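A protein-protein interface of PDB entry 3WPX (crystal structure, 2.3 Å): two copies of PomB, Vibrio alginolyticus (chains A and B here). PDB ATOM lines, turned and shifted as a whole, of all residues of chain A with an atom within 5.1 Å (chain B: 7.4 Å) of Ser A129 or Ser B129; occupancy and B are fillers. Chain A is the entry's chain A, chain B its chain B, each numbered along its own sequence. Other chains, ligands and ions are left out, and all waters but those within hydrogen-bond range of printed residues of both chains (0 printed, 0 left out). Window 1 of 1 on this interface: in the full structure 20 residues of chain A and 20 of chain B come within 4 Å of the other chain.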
ATOM      1  N   ASN A 124      24.650  10.622  21.977  1.00  0.00           N
ATOM      2  CA  ASN A 124      23.561   9.796  21.481  1.00  0.00           C
ATOM      3  C   ASN A 124      23.843   8.306  21.690  1.00  0.00           C
ATOM      4  O   ASN A 124      22.912   7.523  21.890  1.00  0.00           O
ATOM      5  CB  ASN A 124      23.270  10.101  20.002  1.00  0.00           C
ATOM      6  CG  ASN A 124      22.528  11.423  19.808  1.00  0.00           C
ATOM      7  OD1 ASN A 124      21.742  11.837  20.661  1.00  0.00           O
ATOM      8  ND2 ASN A 124      22.783  12.091  18.689  1.00  0.00           N
ATOM      9  N   TRP A 125      25.119   7.921  21.654  1.00  0.00           N
ATOM     10  CA  TRP A 125      25.500   6.549  21.953  1.00  0.00           C
ATOM     11  C   TRP A 125      25.098   6.232  23.384  1.00  0.00           C
ATOM     12  O   TRP A 125      24.613   5.143  23.672  1.00  0.00           O
ATOM     13  CB  TRP A 125      27.010   6.308  21.785  1.00  0.00           C
ATOM     14  CG  TRP A 125      27.508   6.487  20.390  1.00  0.00           C
ATOM     15  CD1 TRP A 125      28.410   7.423  19.957  1.00  0.00           C
ATOM     16  CD2 TRP A 125      27.150   5.713  19.238  1.00  0.00           C
ATOM     17  NE1 TRP A 125      28.629   7.281  18.610  1.00  0.00           N
ATOM     18  CE2 TRP A 125      27.868   6.238  18.139  1.00  0.00           C
ATOM     19  CE3 TRP A 125      26.293   4.623  19.021  1.00  0.00           C
ATOM     20  CZ2 TRP A 125      27.750   5.724  16.849  1.00  0.00           C
ATOM     21  CZ3 TRP A 125      26.178   4.108  17.734  1.00  0.00           C
ATOM     22  CH2 TRP A 125      26.904   4.660  16.666  1.00  0.00           C
ATOM     23  N   ASP A 126      25.317   7.191  24.275  1.00  0.00           N
ATOM     24  CA  ASP A 126      25.004   7.024  25.686  1.00  0.00           C
ATOM     25  C   ASP A 126      23.493   6.910  25.910  1.00  0.00           C
ATOM     26  O   ASP A 126      23.009   5.985  26.555  1.00  0.00           O
ATOM     27  CB  ASP A 126      25.547   8.211  26.481  1.00  0.00           C
ATOM     28  CG  ASP A 126      25.596   7.939  27.971  1.00  0.00           C
ATOM     29  OD1 ASP A 126      25.079   6.884  28.399  1.00  0.00           O
ATOM     30  OD2 ASP A 126      26.150   8.773  28.715  1.00  0.00           O
ATOM     31  N   LEU A 127      22.749   7.859  25.365  1.00  0.00           N
ATOM     32  CA  LEU A 127      21.309   7.889  25.569  1.00  0.00           C
ATOM     33  C   LEU A 127      20.598   6.693  24.917  1.00  0.00           C
ATOM     34  O   LEU A 127      19.738   6.068  25.543  1.00  0.00           O
ATOM     35  CB  LEU A 127      20.733   9.221  25.083  1.00  0.00           C
ATOM     36  CG  LEU A 127      19.211   9.346  24.995  1.00  0.00           C
ATOM     37  CD1 LEU A 127      18.601   9.327  26.391  1.00  0.00           C
ATOM     38  CD2 LEU A 127      18.822  10.622  24.233  1.00  0.00           C
ATOM     39  N   SER A 128      20.952   6.367  23.675  1.00  0.00           N
ATOM     40  CA  SER A 128      20.301   5.247  22.989  1.00  0.00           C
ATOM     41  C   SER A 128      20.641   3.950  23.728  1.00  0.00           C
ATOM     42  O   SER A 128      19.810   3.063  23.911  1.00  0.00           O
ATOM     43  CB  SER A 128      20.718   5.165  21.516  1.00  0.00           C
ATOM     44  OG  SER A 128      22.125   5.020  21.356  1.00  0.00           O
ATOM     45  N   SER A 129      21.878   3.876  24.182  1.00  0.00           N
ATOM     46  CA  SER A 129      22.359   2.733  24.935  1.00  0.00           C
ATOM     47  C   SER A 129      21.582   2.565  26.248  1.00  0.00           C
ATOM     48  O   SER A 129      21.054   1.498  26.529  1.00  0.00           O
ATOM     49  CB  SER A 129      23.851   2.924  25.199  1.00  0.00           C
ATOM     50  OG  SER A 129      24.384   1.801  25.840  1.00  0.00           O
ATOM     51  N   GLN A 130      21.485   3.631  27.034  1.00  0.00           N
ATOM     52  CA  GLN A 130      20.769   3.579  28.302  1.00  0.00           C
ATOM     53  C   GLN A 130      19.282   3.220  28.169  1.00  0.00           C
ATOM     54  O   GLN A 130      18.708   2.571  29.048  1.00  0.00           O
ATOM     55  CB  GLN A 130      20.942   4.896  29.049  1.00  0.00           C
ATOM     56  CG  GLN A 130      22.331   5.065  29.624  1.00  0.00           C
ATOM     57  CD  GLN A 130      22.717   3.900  30.511  1.00  0.00           C
ATOM     58  OE1 GLN A 130      22.127   3.697  31.574  1.00  0.00           O
ATOM     59  NE2 GLN A 130      23.698   3.112  30.071  1.00  0.00           N
ATOM     60  N   ARG A 131      18.655   3.646  27.077  1.00  0.00           N
ATOM     61  CA  ARG A 131      17.252   3.326  26.851  1.00  0.00           C
ATOM     62  C   ARG A 131      17.051   1.836  26.663  1.00  0.00           C
ATOM     63  O   ARG A 131      16.077   1.266  27.170  1.00  0.00           O
ATOM     64  CB  ARG A 131      16.690   4.095  25.654  1.00  0.00           C
ATOM     65  CG  ARG A 131      16.179   5.462  26.050  1.00  0.00           C
ATOM     66  CD  ARG A 131      15.503   6.178  24.910  1.00  0.00           C
ATOM     67  NE  ARG A 131      15.037   7.484  25.337  1.00  0.00           N
ATOM     68  CZ  ARG A 131      14.411   8.351  24.547  1.00  0.00           C
ATOM     69  NH1 ARG A 131      14.191   8.048  23.274  1.00  0.00           N
ATOM     70  NH2 ARG A 131      14.007   9.517  25.033  1.00  0.00           N
ATOM     71  N   ALA A 132      17.971   1.210  25.931  1.00  0.00           N
ATOM     72  CA  ALA A 132      17.923  -0.234  25.740  1.00  0.00           C
ATOM     73  C   ALA A 132      18.199  -0.931  27.066  1.00  0.00           C
ATOM     74  O   ALA A 132      17.622  -1.973  27.338  1.00  0.00           O
ATOM     75  CB  ALA A 132      18.906  -0.688  24.680  1.00  0.00           C
ATOM     76  N   VAL A 133      19.077  -0.346  27.883  1.00  0.00           N
ATOM     77  CA  VAL A 133      19.354  -0.871  29.217  1.00  0.00           C
ATOM     78  C   VAL A 133      18.094  -0.932  30.107  1.00  0.00           C
ATOM     79  O   VAL A 133      17.821  -1.953  30.748  1.00  0.00           O
ATOM     80  CB  VAL A 133      20.481  -0.074  29.924  1.00  0.00           C
ATOM     81  CG1 VAL A 133      20.498  -0.377  31.432  1.00  0.00           C
ATOM     82  CG2 VAL A 133      21.833  -0.378  29.271  1.00  0.00           C
ATOM     83  N   VAL A 152      22.120  -5.944  24.563  1.00  0.00           N
ATOM     84  CA  VAL A 152      21.768  -4.538  24.585  1.00  0.00           C
ATOM     85  C   VAL A 152      22.605  -3.764  23.570  1.00  0.00           C
ATOM     86  O   VAL A 152      23.815  -3.965  23.465  1.00  0.00           O
ATOM     87  CB  VAL A 152      21.923  -3.954  26.006  1.00  0.00           C
ATOM     88  CG1 VAL A 152      22.123  -2.478  25.968  1.00  0.00           C
ATOM     89  CG2 VAL A 152      20.707  -4.307  26.860  1.00  0.00           C
ATOM     90  N   ARG A 153      21.944  -2.890  22.821  1.00  0.00           N
ATOM     91  CA  ARG A 153      22.599  -2.097  21.798  1.00  0.00           C
ATOM     92  C   ARG A 153      22.204  -0.615  21.845  1.00  0.00           C
ATOM     93  O   ARG A 153      21.019  -0.276  21.953  1.00  0.00           O
ATOM     94  CB  ARG A 153      22.230  -2.635  20.418  1.00  0.00           C
ATOM     95  CG  ARG A 153      22.845  -3.963  20.063  1.00  0.00           C
ATOM     96  CD  ARG A 153      22.944  -4.075  18.545  1.00  0.00           C
ATOM     97  NE  ARG A 153      21.656  -3.815  17.905  1.00  0.00           N
ATOM     98  CZ  ARG A 153      21.448  -3.869  16.594  1.00  0.00           C
ATOM     99  NH1 ARG A 153      22.447  -4.171  15.775  1.00  0.00           N
ATOM    100  NH2 ARG A 153      20.244  -3.613  16.101  1.00  0.00           N
ATOM    101  N   GLY A 154      23.198   0.264  21.751  1.00  0.00           N
ATOM    102  CA  GLY A 154      22.958   1.654  21.381  1.00  0.00           C
ATOM    103  C   GLY A 154      23.337   1.905  19.924  1.00  0.00           C
ATOM    104  O   GLY A 154      24.483   1.692  19.521  1.00  0.00           O
ATOM    105  N   ALA B  81      33.185   2.785  34.049  1.00  0.00           N
ATOM    106  CA  ALA B  81      33.197   2.913  32.584  1.00  0.00           C
ATOM    107  C   ALA B  81      34.119   4.043  32.114  1.00  0.00           C
ATOM    108  O   ALA B  81      34.157   4.384  30.928  1.00  0.00           O
ATOM    109  CB  ALA B  81      31.784   3.124  32.053  1.00  0.00           C
ATOM    110  N   VAL B 107      31.584  -2.127  18.903  1.00  0.00           N
ATOM    111  CA  VAL B 107      32.241  -2.075  20.210  1.00  0.00           C
ATOM    112  C   VAL B 107      31.347  -2.715  21.278  1.00  0.00           C
ATOM    113  O   VAL B 107      30.193  -2.345  21.419  1.00  0.00           O
ATOM    114  CB  VAL B 107      32.610  -0.629  20.610  1.00  0.00           C
ATOM    115  CG1 VAL B 107      33.497  -0.615  21.864  1.00  0.00           C
ATOM    116  CG2 VAL B 107      33.314   0.093  19.452  1.00  0.00           C
ATOM    117  N   SER B 108      31.887  -3.698  22.000  1.00  0.00           N
ATOM    118  CA  SER B 108      31.121  -4.483  22.969  1.00  0.00           C
ATOM    119  C   SER B 108      31.800  -4.509  24.326  1.00  0.00           C
ATOM    120  O   SER B 108      32.945  -4.950  24.444  1.00  0.00           O
ATOM    121  CB  SER B 108      30.974  -5.934  22.483  1.00  0.00           C
ATOM    122  OG  SER B 108      30.333  -5.971  21.227  1.00  0.00           O
ATOM    123  N   GLY B 109      31.091  -4.059  25.355  1.00  0.00           N
ATOM    124  CA  GLY B 109      31.581  -4.192  26.720  1.00  0.00           C
ATOM    125  C   GLY B 109      31.102  -5.493  27.330  1.00  0.00           C
ATOM    126  O   GLY B 109      30.055  -6.005  26.942  1.00  0.00           O
ATOM    127  N   HIS B 110      31.869  -6.020  28.279  1.00  0.00           N
ATOM    128  CA  HIS B 110      31.559  -7.280  28.955  1.00  0.00           C
ATOM    129  C   HIS B 110      31.861  -7.155  30.447  1.00  0.00           C
ATOM    130  O   HIS B 110      32.759  -6.411  30.847  1.00  0.00           O
ATOM    131  CB  HIS B 110      32.397  -8.442  28.397  1.00  0.00           C
ATOM    132  CG  HIS B 110      32.197  -8.707  26.938  1.00  0.00           C
ATOM    133  ND1 HIS B 110      31.383  -9.717  26.468  1.00  0.00           N
ATOM    134  CD2 HIS B 110      32.741  -8.119  25.845  1.00  0.00           C
ATOM    135  CE1 HIS B 110      31.414  -9.720  25.146  1.00  0.00           C
ATOM    136  NE2 HIS B 110      32.232  -8.762  24.745  1.00  0.00           N
ATOM    137  N   THR B 111      31.112  -7.888  31.262  1.00  0.00           N
ATOM    138  CA  THR B 111      31.423  -8.041  32.688  1.00  0.00           C
ATOM    139  C   THR B 111      31.577  -9.518  33.065  1.00  0.00           C
ATOM    140  O   THR B 111      31.370 -10.405  32.244  1.00  0.00           O
ATOM    141  CB  THR B 111      30.315  -7.468  33.607  1.00  0.00           C
ATOM    142  OG1 THR B 111      29.109  -8.233  33.462  1.00  0.00           O
ATOM    143  CG2 THR B 111      30.044  -5.997  33.309  1.00  0.00           C
ATOM    144  N   ARG B 122      23.384   0.899  37.147  1.00  0.00           N
ATOM    145  CA  ARG B 122      22.156   0.209  37.543  1.00  0.00           C
ATOM    146  C   ARG B 122      22.294  -1.308  37.483  1.00  0.00           C
ATOM    147  O   ARG B 122      21.569  -2.031  38.158  1.00  0.00           O
ATOM    148  CB  ARG B 122      20.991   0.628  36.645  1.00  0.00           C
ATOM    149  CG  ARG B 122      20.577   2.096  36.761  1.00  0.00           C
ATOM    150  CD  ARG B 122      19.357   2.418  35.889  1.00  0.00           C
ATOM    151  NE  ARG B 122      19.702   2.667  34.489  1.00  0.00           N
ATOM    152  CZ  ARG B 122      18.818   2.740  33.495  1.00  0.00           C
ATOM    153  NH1 ARG B 122      17.522   2.576  33.736  1.00  0.00           N
ATOM    154  NH2 ARG B 122      19.231   2.972  32.252  1.00  0.00           N
ATOM    155  N   SER B 123      23.210  -1.792  36.650  1.00  0.00           N
ATOM    156  CA  SER B 123      23.340  -3.224  36.423  1.00  0.00           C
ATOM    157  C   SER B 123      24.549  -3.483  35.551  1.00  0.00           C
ATOM    158  O   SER B 123      25.222  -2.547  35.120  1.00  0.00           O
ATOM    159  CB  SER B 123      22.091  -3.780  35.732  1.00  0.00           C
ATOM    160  OG  SER B 123      21.953  -3.262  34.415  1.00  0.00           O
ATOM    161  N   ASN B 124      24.818  -4.761  35.299  1.00  0.00           N
ATOM    162  CA  ASN B 124      25.907  -5.157  34.419  1.00  0.00           C
ATOM    163  C   ASN B 124      25.631  -4.796  32.943  1.00  0.00           C
ATOM    164  O   ASN B 124      26.569  -4.606  32.182  1.00  0.00           O
ATOM    165  CB  ASN B 124      26.239  -6.642  34.591  1.00  0.00           C
ATOM    166  CG  ASN B 124      27.202  -6.907  35.767  1.00  0.00           C
ATOM    167  OD1 ASN B 124      27.787  -5.984  36.339  1.00  0.00           O
ATOM    168  ND2 ASN B 124      27.370  -8.180  36.117  1.00  0.00           N
ATOM    169  N   TRP B 125      24.357  -4.695  32.552  1.00  0.00           N
ATOM    170  CA  TRP B 125      24.003  -4.177  31.224  1.00  0.00           C
ATOM    171  C   TRP B 125      24.488  -2.738  31.104  1.00  0.00           C
ATOM    172  O   TRP B 125      25.116  -2.358  30.112  1.00  0.00           O
ATOM    173  CB  TRP B 125      22.482  -4.218  30.978  1.00  0.00           C
ATOM    174  CG  TRP B 125      21.909  -5.599  31.022  1.00  0.00           C
ATOM    175  CD1 TRP B 125      21.023  -6.095  31.939  1.00  0.00           C
ATOM    176  CD2 TRP B 125      22.198  -6.685  30.123  1.00  0.00           C
ATOM    177  NE1 TRP B 125      20.739  -7.409  31.661  1.00  0.00           N
ATOM    178  CE2 TRP B 125      21.450  -7.796  30.551  1.00  0.00           C
ATOM    179  CE3 TRP B 125      23.015  -6.817  28.992  1.00  0.00           C
ATOM    180  CZ2 TRP B 125      21.500  -9.031  29.899  1.00  0.00           C
ATOM    181  CZ3 TRP B 125      23.054  -8.039  28.340  1.00  0.00           C
ATOM    182  CH2 TRP B 125      22.304  -9.130  28.796  1.00  0.00           C
ATOM    183  N   ASP B 126      24.210  -1.952  32.140  1.00  0.00           N
ATOM    184  CA  ASP B 126      24.553  -0.535  32.168  1.00  0.00           C
ATOM    185  C   ASP B 126      26.066  -0.294  32.084  1.00  0.00           C
ATOM    186  O   ASP B 126      26.535   0.446  31.223  1.00  0.00           O
ATOM    187  CB  ASP B 126      24.000   0.123  33.436  1.00  0.00           C
ATOM    188  CG  ASP B 126      24.039   1.657  33.374  1.00  0.00           C
ATOM    189  OD1 ASP B 126      24.333   2.200  32.299  1.00  0.00           O
ATOM    190  OD2 ASP B 126      23.763   2.324  34.391  1.00  0.00           O
ATOM    191  N   LEU B 127      26.809  -0.909  33.004  1.00  0.00           N
ATOM    192  CA  LEU B 127      28.252  -0.766  33.074  1.00  0.00           C
ATOM    193  C   LEU B 127      28.909  -1.252  31.798  1.00  0.00           C
ATOM    194  O   LEU B 127      29.745  -0.552  31.244  1.00  0.00           O
ATOM    195  CB  LEU B 127      28.835  -1.538  34.263  1.00  0.00           C
ATOM    196  CG  LEU B 127      30.368  -1.613  34.242  1.00  0.00           C
ATOM    197  CD1 LEU B 127      31.001  -0.208  34.354  1.00  0.00           C
ATOM    198  CD2 LEU B 127      30.909  -2.534  35.328  1.00  0.00           C
ATOM    199  N   SER B 128      28.537  -2.446  31.334  1.00  0.00           N
ATOM    200  CA  SER B 128      29.167  -3.012  30.142  1.00  0.00           C
ATOM    201  C   SER B 128      28.853  -2.121  28.938  1.00  0.00           C
ATOM    202  O   SER B 128      29.710  -1.866  28.092  1.00  0.00           O
ATOM    203  CB  SER B 128      28.733  -4.467  29.896  1.00  0.00           C
ATOM    204  OG  SER B 128      27.335  -4.595  29.689  1.00  0.00           O
ATOM    205  N   SER B 129      27.617  -1.638  28.902  1.00  0.00           N
ATOM    206  CA  SER B 129      27.156  -0.673  27.922  1.00  0.00           C
ATOM    207  C   SER B 129      27.962   0.625  27.919  1.00  0.00           C
ATOM    208  O   SER B 129      28.428   1.087  26.873  1.00  0.00           O
ATOM    209  CB  SER B 129      25.693  -0.334  28.236  1.00  0.00           C
ATOM    210  OG  SER B 129      24.931  -0.410  27.065  1.00  0.00           O
ATOM    211  N   GLN B 130      28.100   1.233  29.088  1.00  0.00           N
ATOM    212  CA  GLN B 130      28.819   2.493  29.197  1.00  0.00           C
ATOM    213  C   GLN B 130      30.302   2.373  28.829  1.00  0.00           C
ATOM    214  O   GLN B 130      30.915   3.332  28.363  1.00  0.00           O
ATOM    215  CB  GLN B 130      28.639   3.078  30.595  1.00  0.00           C
ATOM    216  CG  GLN B 130      27.283   3.739  30.774  1.00  0.00           C
ATOM    217  CD  GLN B 130      27.041   4.830  29.746  1.00  0.00           C
ATOM    218  OE1 GLN B 130      27.810   5.795  29.657  1.00  0.00           O
ATOM    219  NE2 GLN B 130      25.985   4.673  28.944  1.00  0.00           N
ATOM    220  N   ARG B 131      30.881   1.192  29.033  1.00  0.00           N
ATOM    221  CA  ARG B 131      32.271   0.985  28.661  1.00  0.00           C
ATOM    222  C   ARG B 131      32.420   1.053  27.157  1.00  0.00           C
ATOM    223  O   ARG B 131      33.394   1.599  26.651  1.00  0.00           O
ATOM    224  CB  ARG B 131      32.799  -0.353  29.190  1.00  0.00           C
ATOM    225  CG  ARG B 131      33.115  -0.286  30.656  1.00  0.00           C
ATOM    226  CD  ARG B 131      33.896  -1.496  31.143  1.00  0.00           C
ATOM    227  NE  ARG B 131      34.510  -1.202  32.432  1.00  0.00           N
ATOM    228  CZ  ARG B 131      35.196  -2.078  33.151  1.00  0.00           C
ATOM    229  NH1 ARG B 131      35.347  -3.320  32.715  1.00  0.00           N
ATOM    230  NH2 ARG B 131      35.727  -1.710  34.309  1.00  0.00           N
ATOM    231  N   ALA B 132      31.448   0.490  26.447  1.00  0.00           N
ATOM    232  CA  ALA B 132      31.469   0.487  24.990  1.00  0.00           C
ATOM    233  C   ALA B 132      31.217   1.893  24.465  1.00  0.00           C
ATOM    234  O   ALA B 132      31.738   2.279  23.419  1.00  0.00           O
ATOM    235  CB  ALA B 132      30.436  -0.489  24.437  1.00  0.00           C
ATOM    236  N   VAL B 133      30.412   2.654  25.201  1.00  0.00           N
ATOM    237  CA  VAL B 133      30.184   4.049  24.877  1.00  0.00           C
ATOM    238  C   VAL B 133      31.482   4.861  25.015  1.00  0.00           C
ATOM    239  O   VAL B 133      31.818   5.635  24.138  1.00  0.00           O
ATOM    240  CB  VAL B 133      29.069   4.674  25.746  1.00  0.00           C
ATOM    241  CG1 VAL B 133      29.027   6.189  25.544  1.00  0.00           C
ATOM    242  CG2 VAL B 133      27.713   4.053  25.400  1.00  0.00           C
ATOM    243  N   SER B 134      32.216   4.666  26.105  1.00  0.00           N
ATOM    244  CA  SER B 134      33.464   5.394  26.308  1.00  0.00           C
ATOM    245  C   SER B 134      34.442   5.163  25.162  1.00  0.00           C
ATOM    246  O   SER B 134      35.044   6.099  24.647  1.00  0.00           O
ATOM    247  CB  SER B 134      34.101   5.000  27.631  1.00  0.00           C
ATOM    248  OG  SER B 134      33.287   5.422  28.713  1.00  0.00           O
ATOM    249  N   VAL B 135      34.579   3.909  24.750  1.00  0.00           N
ATOM    250  CA  VAL B 135      35.485   3.555  23.664  1.00  0.00           C
ATOM    251  C   VAL B 135      35.021   4.153  22.326  1.00  0.00           C
ATOM    252  O   VAL B 135      35.803   4.792  21.626  1.00  0.00           O
ATOM    253  CB  VAL B 135      35.680   2.026  23.582  1.00  0.00           C
ATOM    254  CG1 VAL B 135      36.502   1.643  22.353  1.00  0.00           C
ATOM    255  CG2 VAL B 135      36.352   1.512  24.864  1.00  0.00           C
ATOM    256  N   VAL B 152      27.260   0.112  19.306  1.00  0.00           N
ATOM    257  CA  VAL B 152      27.578  -0.061  20.715  1.00  0.00           C
ATOM    258  C   VAL B 152      26.721  -1.168  21.321  1.00  0.00           C
ATOM    259  O   VAL B 152      25.525  -1.220  21.079  1.00  0.00           O
ATOM    260  CB  VAL B 152      27.354   1.245  21.492  1.00  0.00           C
ATOM    261  CG1 VAL B 152      27.494   0.996  22.964  1.00  0.00           C
ATOM    262  CG2 VAL B 152      28.345   2.320  21.026  1.00  0.00           C
ATOM    263  N   ARG B 153      27.341  -2.073  22.077  1.00  0.00           N
ATOM    264  CA  ARG B 153      26.611  -3.152  22.731  1.00  0.00           C
ATOM    265  C   ARG B 153      27.110  -3.369  24.147  1.00  0.00           C
ATOM    266  O   ARG B 153      28.295  -3.201  24.434  1.00  0.00           O
ATOM    267  CB  ARG B 153      26.754  -4.480  21.987  1.00  0.00           C
ATOM    268  CG  ARG B 153      26.672  -4.421  20.487  1.00  0.00           C
ATOM    269  CD  ARG B 153      27.486  -5.585  19.916  1.00  0.00           C
ATOM    270  NE  ARG B 153      26.795  -6.875  19.950  1.00  0.00           N
ATOM    271  CZ  ARG B 153      27.397  -8.057  20.102  1.00  0.00           C
ATOM    272  NH1 ARG B 153      28.709  -8.145  20.271  1.00  0.00           N
ATOM    273  NH2 ARG B 153      26.672  -9.163  20.103  1.00  0.00           N
ATOM    274  N   GLY B 154      26.185  -3.724  25.028  1.00  0.00           N
ATOM    275  CA  GLY B 154      26.515  -4.202  26.356  1.00  0.00           C
ATOM    276  C   GLY B 154      26.123  -5.667  26.447  1.00  0.00           C
ATOM    277  O   GLY B 154      24.978  -6.027  26.191  1.00  0.00           O
ATOM    278  N   MET B 155      27.070  -6.520  26.813  1.00  0.00           N
ATOM    279  CA  MET B 155      26.817  -7.948  26.807  1.00  0.00           C
ATOM    280  C   MET B 155      26.657  -8.490  28.213  1.00  0.00           C
ATOM    281  O   MET B 155      26.329  -9.664  28.389  1.00  0.00           O
ATOM    282  CB  MET B 155      27.960  -8.687  26.088  1.00  0.00           C
ATOM    283  CG  MET B 155      28.291  -8.131  24.692  1.00  0.00           C
ATOM    284  SD  MET B 155      26.977  -8.397  23.491  1.00  0.00           S
ATOM    285  CE  MET B 155      27.113 -10.169  23.314  1.00  0.00           C
ATOM    286  N   ALA B 156      26.876  -7.632  29.206  1.00  0.00           N
ATOM    287  CA  ALA B 156      26.933  -8.074  30.592  1.00  0.00           C
ATOM    288  C   ALA B 156      27.812  -9.326  30.657  1.00  0.00           C
ATOM    289  O   ALA B 156      28.913  -9.337  30.116  1.00  0.00           O
ATOM    290  CB  ALA B 156      25.523  -8.351  31.142  1.00  0.00           C
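Val A133 touches Asp B126, but with the chains exchanged Asp A126 does not touch Val B133 (4.03 Å). Val A133 touches Ser B129, but with the chains exchanged Ser A129 does not touch Val B133 (4.03 Å). Val A152 touches Ser B129, but with the chains exchanged Ser A129 does not touch Val B152 (4.3 Å). Val A152 touches Gly B154, and with the chains exchanged Gly A154 touches Val B152.
Hydrophobic or aromatic side chains of chain A that line the printed part of chain B: Trp A125, Val A133 and Val A152.
Among the printed residues, pairs that only touch across the chains: Val A152 with Arg B153, Arg A153 with Val B152, Val A152 with Ser B129, Val A133 with Arg B122, Trp A125 with Val B152, Trp A125 with Val B133, Val A133 with Ser B129, Arg A153 with Arg B153, Val A133 with Trp B125 and Val A133 with Asp B126.
The backbone NH (N) of Arg B153 sits at hydrogen-bond distance from the backbone carbonyl oxygen (O) of Val B107 (2.9 Å). The side-chain hydroxyl (OG) of Ser B108 sits at hydrogen-bond distance from the guanidinium group (NH1) of Arg B153, 2.9 Å away. N of Arg B122 lies within hydrogen-bond range of OD2 of Asp B126, at 3.1 Å. N of Asp B126 lies within hydrogen-bond range of OG of Ser B123 (3.5 Å). The side-chain hydroxyl (OG) of Ser B128 lies within hydrogen-bond range of the backbone carbonyl oxygen (O) of Trp B125, at 3.2 Å. The side-chain hydroxyl (OG) of Ser B134 lies within hydrogen-bond range of the backbone carbonyl oxygen (O) of Gln B130, 3.2 Å away.
Printed residues of chain B within 4 Å of Ser A129: Ser B129 (2.6 Å). Ser B129 touches just these residues of chain A: Ser A129, Val A133 and Val A152. No residue of chain B comes within 4 Å of Ser A128. Of the printed residues of chain B, Arg A153 touches Val B152 (3.1 Å) and Arg B153 (3.9 Å). Of the printed residues of chain A, Trp B125 touches Val A133. Of the printed residues of chain A, Arg B122 touches Gln A130 and Val A133. Printed residues of chain A within 4 Å of Asp B126: Gln A130 and Val A133. Ser B128 touches none of the printed residues of chain A. His B110 touches none of the printed residues of chain A.
The side-chain carboxylate of Asp A126 sits at hydrogen-bond distance from the side-chain amide nitrogen of Gln B130, 2.5 Å away. The side-chain hydroxyl (OG) of Ser B129 sits at hydrogen-bond distance from the side-chain hydroxyl (OG) of Ser A129. OE1 of Gln A130 sits at hydrogen-bond distance from NH2 of Arg B122 (3.1 Å). The side-chain carboxylate (OD1) of Asp B126 is in hydrogen-bond range of the side-chain amide nitrogen (NE2) of Gln A130 (2.5 Å). The side-chain amide nitrogen (NE2) of Gln B130 lies close to the side-chain amide nitrogen (NE2) of Gln A130. O of Val A152 is in hydrogen-bond range of N of Gly B154, at 2.8 Å. The backbone NH (N) of Gly A154 is in hydrogen-bond range of the backbone carbonyl oxygen (O) of Val B152.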
